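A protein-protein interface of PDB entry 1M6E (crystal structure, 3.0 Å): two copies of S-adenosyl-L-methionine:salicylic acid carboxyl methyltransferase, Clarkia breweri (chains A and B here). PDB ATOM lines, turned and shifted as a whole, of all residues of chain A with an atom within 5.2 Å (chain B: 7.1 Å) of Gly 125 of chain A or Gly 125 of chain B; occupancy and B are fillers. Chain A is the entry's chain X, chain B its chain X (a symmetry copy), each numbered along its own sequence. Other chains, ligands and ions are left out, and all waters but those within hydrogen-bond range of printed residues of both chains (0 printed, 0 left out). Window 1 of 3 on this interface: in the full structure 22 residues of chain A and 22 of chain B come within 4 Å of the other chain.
The backbone NH (N) of Gly 125 of chain B lies within hydrogen-bond range of the backbone carbonyl oxygen (O) of Gly 125 of chain A (3.0 Å).
N of Leu 96 of chain A sits at hydrogen-bond distance from O of Asn 124 of chain A (2.7 Å).
The backbone carbonyl oxygen (O) of Leu 96 of chain A lies within hydrogen-bond range of the backbone NH (N) of Val 126 of chain A, at 2.7 Å.
O of Ile 94 of chain B is in hydrogen-bond range of N of Asn 124 of chain B.
The backbone NH of Leu 96 of chain B is in hydrogen-bond range of the backbone carbonyl oxygen of Asn 124 of chain B (2.7 Å).
N of Val 126 of chain B sits at hydrogen-bond distance from O of Leu 96 of chain B (2.7 Å).
ND2 of Asn 97 of chain B is in hydrogen-bond range of O of Val 126 of chain B (2.9 Å).
Phe 108 of chain B touches Phe 104 of chain A.
Phe 108 of chain A touches Phe 104 of chain B (CD1 to CD1, 3.7 Å).
O of Gly 125 of chain B touches CZ of Phe 108 of chain A, at 3.996 Å.
CG of Pro 127 of chain B touches CG of Phe 108 of chain A (3.3 Å).
Val 126 of chain B touches Ile 123 of chain A.
Phe 95 of chain B touches Asn 124 of chain A (CE2 to OD1, 3.98 Å).
Gly 125 of chain A touches Phe 108 of chain B.
O of Ile 123 of chain B touches CA of Val 126 of chain A, 3.9 Å away.
OD1 of Asn 124 of chain B touches CG2 of Val 126 of chain A, at 2.9 Å.
Pro 127 of chain A touches Phe 108 of chain B (CG to CG, 3.3 Å).
Leu 96 of chain A touches none of the printed residues of chain B.
Of the printed residues of chain B, Phe 108 of chain A touches Phe 104 (3.7 Å), Gly 125 (3.996 Å) and Pro 127 (3.3 Å).
Of the printed residues of chain B, Gly 125 of chain A touches Phe 108, Asn 124 and Gly 125.
Asp 98 of chain B touches none of the printed residues of chain A.
Printed residues of chain A within 4 Å of Phe 108 of chain B: Phe 104, Gly 125 and Pro 127.
Of the printed residues of chain A, Gly 125 of chain B touches Phe 108 (3.996 Å), Asn 124 (3.4 Å) and Gly 125 (3.0 Å).
Printed residues of chain A within 4 Å of Val 126 of chain B: Ile 123 (3.9 Å) and Asn 124 (2.9 Å).
The nearest printed residue of chain A that does not touch Gly 125 of chain B is Ile 123 of chain A (4.2 Å).
The nearest printed residue of chain A that does not touch Phe 108 of chain B is Phe 108 of chain A (4.1 Å).
Of the 8 printed residues of chain A, 7 touch a printed residue of chain B.
Printed residues of chain A that touch a printed residue of chain B: Phe 104, Phe 108, Ile 123, Asn 124, Gly 125, Val 126 and Pro 127.
Hydrophobic or aromatic side chains of chain B that line the printed part of chain A: Phe 95, Phe 104, Phe 108, Val 126 and Pro 127.
Among the printed residues, 16 pairs touch across the chains.
Phe 108 of chain A touches Gly 125 of chain B, and with the chains exchanged Gly 125 of chain A touches Phe 108 of chain B.
Phe 108 of chain A touches Pro 127 of chain B, and with the chains exchanged Pro 127 of chain A touches Phe 108 of chain B.
Ile 123 of chain A touches Val 126 of chain B, and with the chains exchanged Val 126 of chain A touches Ile 123 of chain B.
Ile 123 of chain A touches Pro 127 of chain B, and with the chains exchanged Pro 127 of chain A touches Ile 123 of chain B.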
ATOM      1  N   LEU A  96      27.227   6.305 -15.629  1.00  0.00           N
ATOM      2  CA  LEU A  96      28.670   6.262 -15.900  1.00  0.00           C
ATOM      3  C   LEU A  96      29.220   5.066 -15.145  1.00  0.00           C
ATOM      4  O   LEU A  96      29.198   5.032 -13.904  1.00  0.00           O
ATOM      5  CB  LEU A  96      29.367   7.511 -15.400  1.00  0.00           C
ATOM      6  CG  LEU A  96      28.808   8.844 -15.872  1.00  0.00           C
ATOM      7  CD1 LEU A  96      29.597   9.937 -15.230  1.00  0.00           C
ATOM      8  CD2 LEU A  96      28.828   8.941 -17.390  1.00  0.00           C
ATOM      9  N   PHE A 104      35.702   8.297  -9.619  1.00  0.00           N
ATOM     10  CA  PHE A 104      34.331   8.794  -9.661  1.00  0.00           C
ATOM     11  C   PHE A 104      34.228  10.132  -8.977  1.00  0.00           C
ATOM     12  O   PHE A 104      33.478  10.979  -9.419  1.00  0.00           O
ATOM     13  CB  PHE A 104      33.375   7.787  -9.045  1.00  0.00           C
ATOM     14  CG  PHE A 104      33.093   6.609  -9.946  1.00  0.00           C
ATOM     15  CD1 PHE A 104      33.867   5.467  -9.881  1.00  0.00           C
ATOM     16  CD2 PHE A 104      32.105   6.686 -10.919  1.00  0.00           C
ATOM     17  CE1 PHE A 104      33.667   4.441 -10.765  1.00  0.00           C
ATOM     18  CE2 PHE A 104      31.899   5.655 -11.814  1.00  0.00           C
ATOM     19  CZ  PHE A 104      32.673   4.537 -11.744  1.00  0.00           C
ATOM     20  N   PHE A 108      32.323  13.397 -10.390  1.00  0.00           N
ATOM     21  CA  PHE A 108      31.271  13.997  -9.604  1.00  0.00           C
ATOM     22  C   PHE A 108      31.621  15.419  -9.211  1.00  0.00           C
ATOM     23  O   PHE A 108      30.732  16.288  -9.065  1.00  0.00           O
ATOM     24  CB  PHE A 108      31.009  13.143  -8.372  1.00  0.00           C
ATOM     25  CG  PHE A 108      30.383  11.818  -8.688  1.00  0.00           C
ATOM     26  CD1 PHE A 108      30.293  10.829  -7.715  1.00  0.00           C
ATOM     27  CD2 PHE A 108      29.959  11.522  -9.997  1.00  0.00           C
ATOM     28  CE1 PHE A 108      29.803   9.566  -8.043  1.00  0.00           C
ATOM     29  CE2 PHE A 108      29.475  10.282 -10.317  1.00  0.00           C
ATOM     30  CZ  PHE A 108      29.397   9.292  -9.337  1.00  0.00           C
ATOM     31  N   ILE A 123      22.686  12.391 -13.390  1.00  0.00           N
ATOM     32  CA  ILE A 123      23.855  11.532 -13.531  1.00  0.00           C
ATOM     33  C   ILE A 123      24.047  10.556 -12.395  1.00  0.00           C
ATOM     34  O   ILE A 123      23.864  10.899 -11.231  1.00  0.00           O
ATOM     35  CB  ILE A 123      25.143  12.329 -13.700  1.00  0.00           C
ATOM     36  CG1 ILE A 123      25.117  13.026 -15.058  1.00  0.00           C
ATOM     37  CG2 ILE A 123      26.348  11.390 -13.601  1.00  0.00           C
ATOM     38  CD1 ILE A 123      26.287  13.888 -15.332  1.00  0.00           C
ATOM     39  N   ASN A 124      24.417   9.334 -12.759  1.00  0.00           N
ATOM     40  CA  ASN A 124      24.626   8.264 -11.806  1.00  0.00           C
ATOM     41  C   ASN A 124      25.892   7.495 -12.143  1.00  0.00           C
ATOM     42  O   ASN A 124      26.080   7.095 -13.298  1.00  0.00           O
ATOM     43  CB  ASN A 124      23.441   7.282 -11.830  1.00  0.00           C
ATOM     44  CG  ASN A 124      22.096   7.964 -11.610  1.00  0.00           C
ATOM     45  OD1 ASN A 124      21.864   8.589 -10.580  1.00  0.00           O
ATOM     46  ND2 ASN A 124      21.202   7.837 -12.580  1.00  0.00           N
ATOM     47  N   GLY A 125      26.754   7.296 -11.142  1.00  0.00           N
ATOM     48  CA  GLY A 125      27.970   6.499 -11.310  1.00  0.00           C
ATOM     49  C   GLY A 125      27.657   5.050 -10.896  1.00  0.00           C
ATOM     50  O   GLY A 125      27.116   4.835  -9.836  1.00  0.00           O
ATOM     51  N   VAL A 126      27.960   4.068 -11.737  1.00  0.00           N
ATOM     52  CA  VAL A 126      27.676   2.650 -11.456  1.00  0.00           C
ATOM     53  C   VAL A 126      28.974   1.849 -11.339  1.00  0.00           C
ATOM     54  O   VAL A 126      29.482   1.348 -12.337  1.00  0.00           O
ATOM     55  CB  VAL A 126      26.917   2.037 -12.618  1.00  0.00           C
ATOM     56  CG1 VAL A 126      26.748   0.580 -12.393  1.00  0.00           C
ATOM     57  CG2 VAL A 126      25.618   2.742 -12.813  1.00  0.00           C
ATOM     58  N   PRO A 127      29.520   1.679 -10.129  1.00  0.00           N
ATOM     59  CA  PRO A 127      30.777   0.905 -10.113  1.00  0.00           C
ATOM     60  C   PRO A 127      30.659  -0.627 -10.310  1.00  0.00           C
ATOM     61  O   PRO A 127      29.824  -1.277  -9.683  1.00  0.00           O
ATOM     62  CB  PRO A 127      31.396   1.290  -8.766  1.00  0.00           C
ATOM     63  CG  PRO A 127      30.196   1.480  -7.907  1.00  0.00           C
ATOM     64  CD  PRO A 127      29.195   2.205  -8.790  1.00  0.00           C
ATOM     65  N   CYS B  60      23.611   9.995   2.292  1.00  0.00           N
ATOM     66  CA  CYS B  60      24.338   8.827   2.807  1.00  0.00           C
ATOM     67  C   CYS B  60      25.702   9.412   3.034  1.00  0.00           C
ATOM     68  O   CYS B  60      25.856  10.623   2.982  1.00  0.00           O
ATOM     69  CB  CYS B  60      24.441   7.733   1.734  1.00  0.00           C
ATOM     70  SG  CYS B  60      25.385   8.217   0.216  1.00  0.00           S
ATOM     71  N   ILE B  94      19.603   0.412  -6.057  1.00  0.00           N
ATOM     72  CA  ILE B  94      20.003   1.391  -5.075  1.00  0.00           C
ATOM     73  C   ILE B  94      20.641   2.686  -5.549  1.00  0.00           C
ATOM     74  O   ILE B  94      21.474   2.715  -6.453  1.00  0.00           O
ATOM     75  CB  ILE B  94      20.932   0.734  -4.100  1.00  0.00           C
ATOM     76  CG1 ILE B  94      20.264  -0.515  -3.559  1.00  0.00           C
ATOM     77  CG2 ILE B  94      21.300   1.707  -3.006  1.00  0.00           C
ATOM     78  CD1 ILE B  94      21.119  -1.206  -2.532  1.00  0.00           C
ATOM     79  N   PHE B  95      20.241   3.761  -4.890  1.00  0.00           N
ATOM     80  CA  PHE B  95      20.749   5.081  -5.197  1.00  0.00           C
ATOM     81  C   PHE B  95      21.314   5.761  -3.964  1.00  0.00           C
ATOM     82  O   PHE B  95      20.540   6.148  -3.084  1.00  0.00           O
ATOM     83  CB  PHE B  95      19.620   5.917  -5.784  1.00  0.00           C
ATOM     84  CG  PHE B  95      19.246   5.507  -7.166  1.00  0.00           C
ATOM     85  CD1 PHE B  95      18.117   4.751  -7.399  1.00  0.00           C
ATOM     86  CD2 PHE B  95      20.088   5.806  -8.234  1.00  0.00           C
ATOM     87  CE1 PHE B  95      17.835   4.287  -8.687  1.00  0.00           C
ATOM     88  CE2 PHE B  95      19.820   5.352  -9.509  1.00  0.00           C
ATOM     89  CZ  PHE B  95      18.696   4.591  -9.739  1.00  0.00           C
ATOM     90  N   LEU B  96      22.646   5.894  -3.902  1.00  0.00           N
ATOM     91  CA  LEU B  96      23.332   6.544  -2.779  1.00  0.00           C
ATOM     92  C   LEU B  96      23.605   7.975  -3.204  1.00  0.00           C
ATOM     93  O   LEU B  96      24.377   8.223  -4.144  1.00  0.00           O
ATOM     94  CB  LEU B  96      24.654   5.871  -2.469  1.00  0.00           C
ATOM     95  CG  LEU B  96      24.621   4.369  -2.235  1.00  0.00           C
ATOM     96  CD1 LEU B  96      26.020   3.900  -2.000  1.00  0.00           C
ATOM     97  CD2 LEU B  96      23.699   4.015  -1.078  1.00  0.00           C
ATOM     98  N   ASN B  97      22.952   8.909  -2.512  1.00  0.00           N
ATOM     99  CA  ASN B  97      23.065  10.323  -2.811  1.00  0.00           C
ATOM    100  C   ASN B  97      23.752  11.202  -1.796  1.00  0.00           C
ATOM    101  O   ASN B  97      23.546  11.113  -0.578  1.00  0.00           O
ATOM    102  CB  ASN B  97      21.691  10.936  -3.076  1.00  0.00           C
ATOM    103  CG  ASN B  97      21.694  12.464  -2.923  1.00  0.00           C
ATOM    104  OD1 ASN B  97      21.420  13.019  -1.841  1.00  0.00           O
ATOM    105  ND2 ASN B  97      22.024  13.143  -4.004  1.00  0.00           N
ATOM    106  N   ASP B  98      24.570  12.087  -2.320  1.00  0.00           N
ATOM    107  CA  ASP B  98      25.201  13.009  -1.448  1.00  0.00           C
ATOM    108  C   ASP B  98      25.716  14.134  -2.269  1.00  0.00           C
ATOM    109  O   ASP B  98      25.600  14.090  -3.499  1.00  0.00           O
ATOM    110  CB  ASP B  98      26.299  12.351  -0.652  1.00  0.00           C
ATOM    111  CG  ASP B  98      26.592  13.113   0.607  1.00  0.00           C
ATOM    112  OD1 ASP B  98      27.030  14.274   0.464  1.00  0.00           O
ATOM    113  OD2 ASP B  98      26.363  12.582   1.718  1.00  0.00           O
ATOM    114  N   PHE B 104      32.612   9.164  -2.524  1.00  0.00           N
ATOM    115  CA  PHE B 104      31.976   8.094  -3.286  1.00  0.00           C
ATOM    116  C   PHE B 104      32.970   7.010  -3.613  1.00  0.00           C
ATOM    117  O   PHE B 104      32.616   5.849  -3.614  1.00  0.00           O
ATOM    118  CB  PHE B 104      31.328   8.644  -4.545  1.00  0.00           C
ATOM    119  CG  PHE B 104      30.032   9.372  -4.275  1.00  0.00           C
ATOM    120  CD1 PHE B 104      30.022  10.731  -4.035  1.00  0.00           C
ATOM    121  CD2 PHE B 104      28.837   8.671  -4.178  1.00  0.00           C
ATOM    122  CE1 PHE B 104      28.858  11.369  -3.698  1.00  0.00           C
ATOM    123  CE2 PHE B 104      27.661   9.308  -3.837  1.00  0.00           C
ATOM    124  CZ  PHE B 104      27.664  10.648  -3.595  1.00  0.00           C
ATOM    125  N   PHE B 108      32.396   3.038  -3.193  1.00  0.00           N
ATOM    126  CA  PHE B 108      32.537   2.178  -4.344  1.00  0.00           C
ATOM    127  C   PHE B 108      33.657   1.176  -4.148  1.00  0.00           C
ATOM    128  O   PHE B 108      33.608   0.039  -4.671  1.00  0.00           O
ATOM    129  CB  PHE B 108      32.779   3.027  -5.585  1.00  0.00           C
ATOM    130  CG  PHE B 108      31.585   3.832  -5.998  1.00  0.00           C
ATOM    131  CD1 PHE B 108      31.702   4.829  -6.960  1.00  0.00           C
ATOM    132  CD2 PHE B 108      30.345   3.653  -5.355  1.00  0.00           C
ATOM    133  CE1 PHE B 108      30.611   5.640  -7.265  1.00  0.00           C
ATOM    134  CE2 PHE B 108      29.273   4.449  -5.659  1.00  0.00           C
ATOM    135  CZ  PHE B 108      29.403   5.453  -6.618  1.00  0.00           C
ATOM    136  N   ILE B 123      24.116  -1.069  -7.372  1.00  0.00           N
ATOM    137  CA  ILE B 123      24.344   0.189  -6.672  1.00  0.00           C
ATOM    138  C   ILE B 123      24.745   1.334  -7.570  1.00  0.00           C
ATOM    139  O   ILE B 123      25.543   1.166  -8.488  1.00  0.00           O
ATOM    140  CB  ILE B 123      25.387   0.057  -5.569  1.00  0.00           C
ATOM    141  CG1 ILE B 123      24.816  -0.811  -4.450  1.00  0.00           C
ATOM    142  CG2 ILE B 123      25.754   1.445  -5.037  1.00  0.00           C
ATOM    143  CD1 ILE B 123      25.749  -1.072  -3.333  1.00  0.00           C
ATOM    144  N   ASN B 124      24.175   2.499  -7.287  1.00  0.00           N
ATOM    145  CA  ASN B 124      24.426   3.700  -8.055  1.00  0.00           C
ATOM    146  C   ASN B 124      24.627   4.888  -7.130  1.00  0.00           C
ATOM    147  O   ASN B 124      23.814   5.109  -6.226  1.00  0.00           O
ATOM    148  CB  ASN B 124      23.235   4.004  -8.983  1.00  0.00           C
ATOM    149  CG  ASN B 124      22.870   2.834  -9.888  1.00  0.00           C
ATOM    150  OD1 ASN B 124      23.680   2.374 -10.686  1.00  0.00           O
ATOM    151  ND2 ASN B 124      21.640   2.355  -9.769  1.00  0.00           N
ATOM    152  N   GLY B 125      25.708   5.642  -7.352  1.00  0.00           N
ATOM    153  CA  GLY B 125      25.975   6.862  -6.590  1.00  0.00           C
ATOM    154  C   GLY B 125      25.385   8.053  -7.366  1.00  0.00           C
ATOM    155  O   GLY B 125      25.640   8.187  -8.540  1.00  0.00           O
ATOM    156  N   VAL B 126      24.577   8.891  -6.727  1.00  0.00           N
ATOM    157  CA  VAL B 126      23.933  10.044  -7.380  1.00  0.00           C
ATOM    158  C   VAL B 126      24.432  11.358  -6.777  1.00  0.00           C
ATOM    159  O   VAL B 126      23.869  11.843  -5.802  1.00  0.00           O
ATOM    160  CB  VAL B 126      22.439  10.014  -7.121  1.00  0.00           C
ATOM    161  CG1 VAL B 126      21.811  11.243  -7.666  1.00  0.00           C
ATOM    162  CG2 VAL B 126      21.843   8.768  -7.685  1.00  0.00           C
ATOM    163  N   PRO B 127      25.468  11.979  -7.353  1.00  0.00           N
ATOM    164  CA  PRO B 127      25.890  13.232  -6.697  1.00  0.00           C
ATOM    165  C   PRO B 127      24.987  14.473  -6.909  1.00  0.00           C
ATOM    166  O   PRO B 127      24.583  14.769  -8.032  1.00  0.00           O
ATOM    167  CB  PRO B 127      27.314  13.430  -7.225  1.00  0.00           C
ATOM    168  CG  PRO B 127      27.223  12.872  -8.602  1.00  0.00           C
ATOM    169  CD  PRO B 127      26.375  11.620  -8.459  1.00  0.00           C
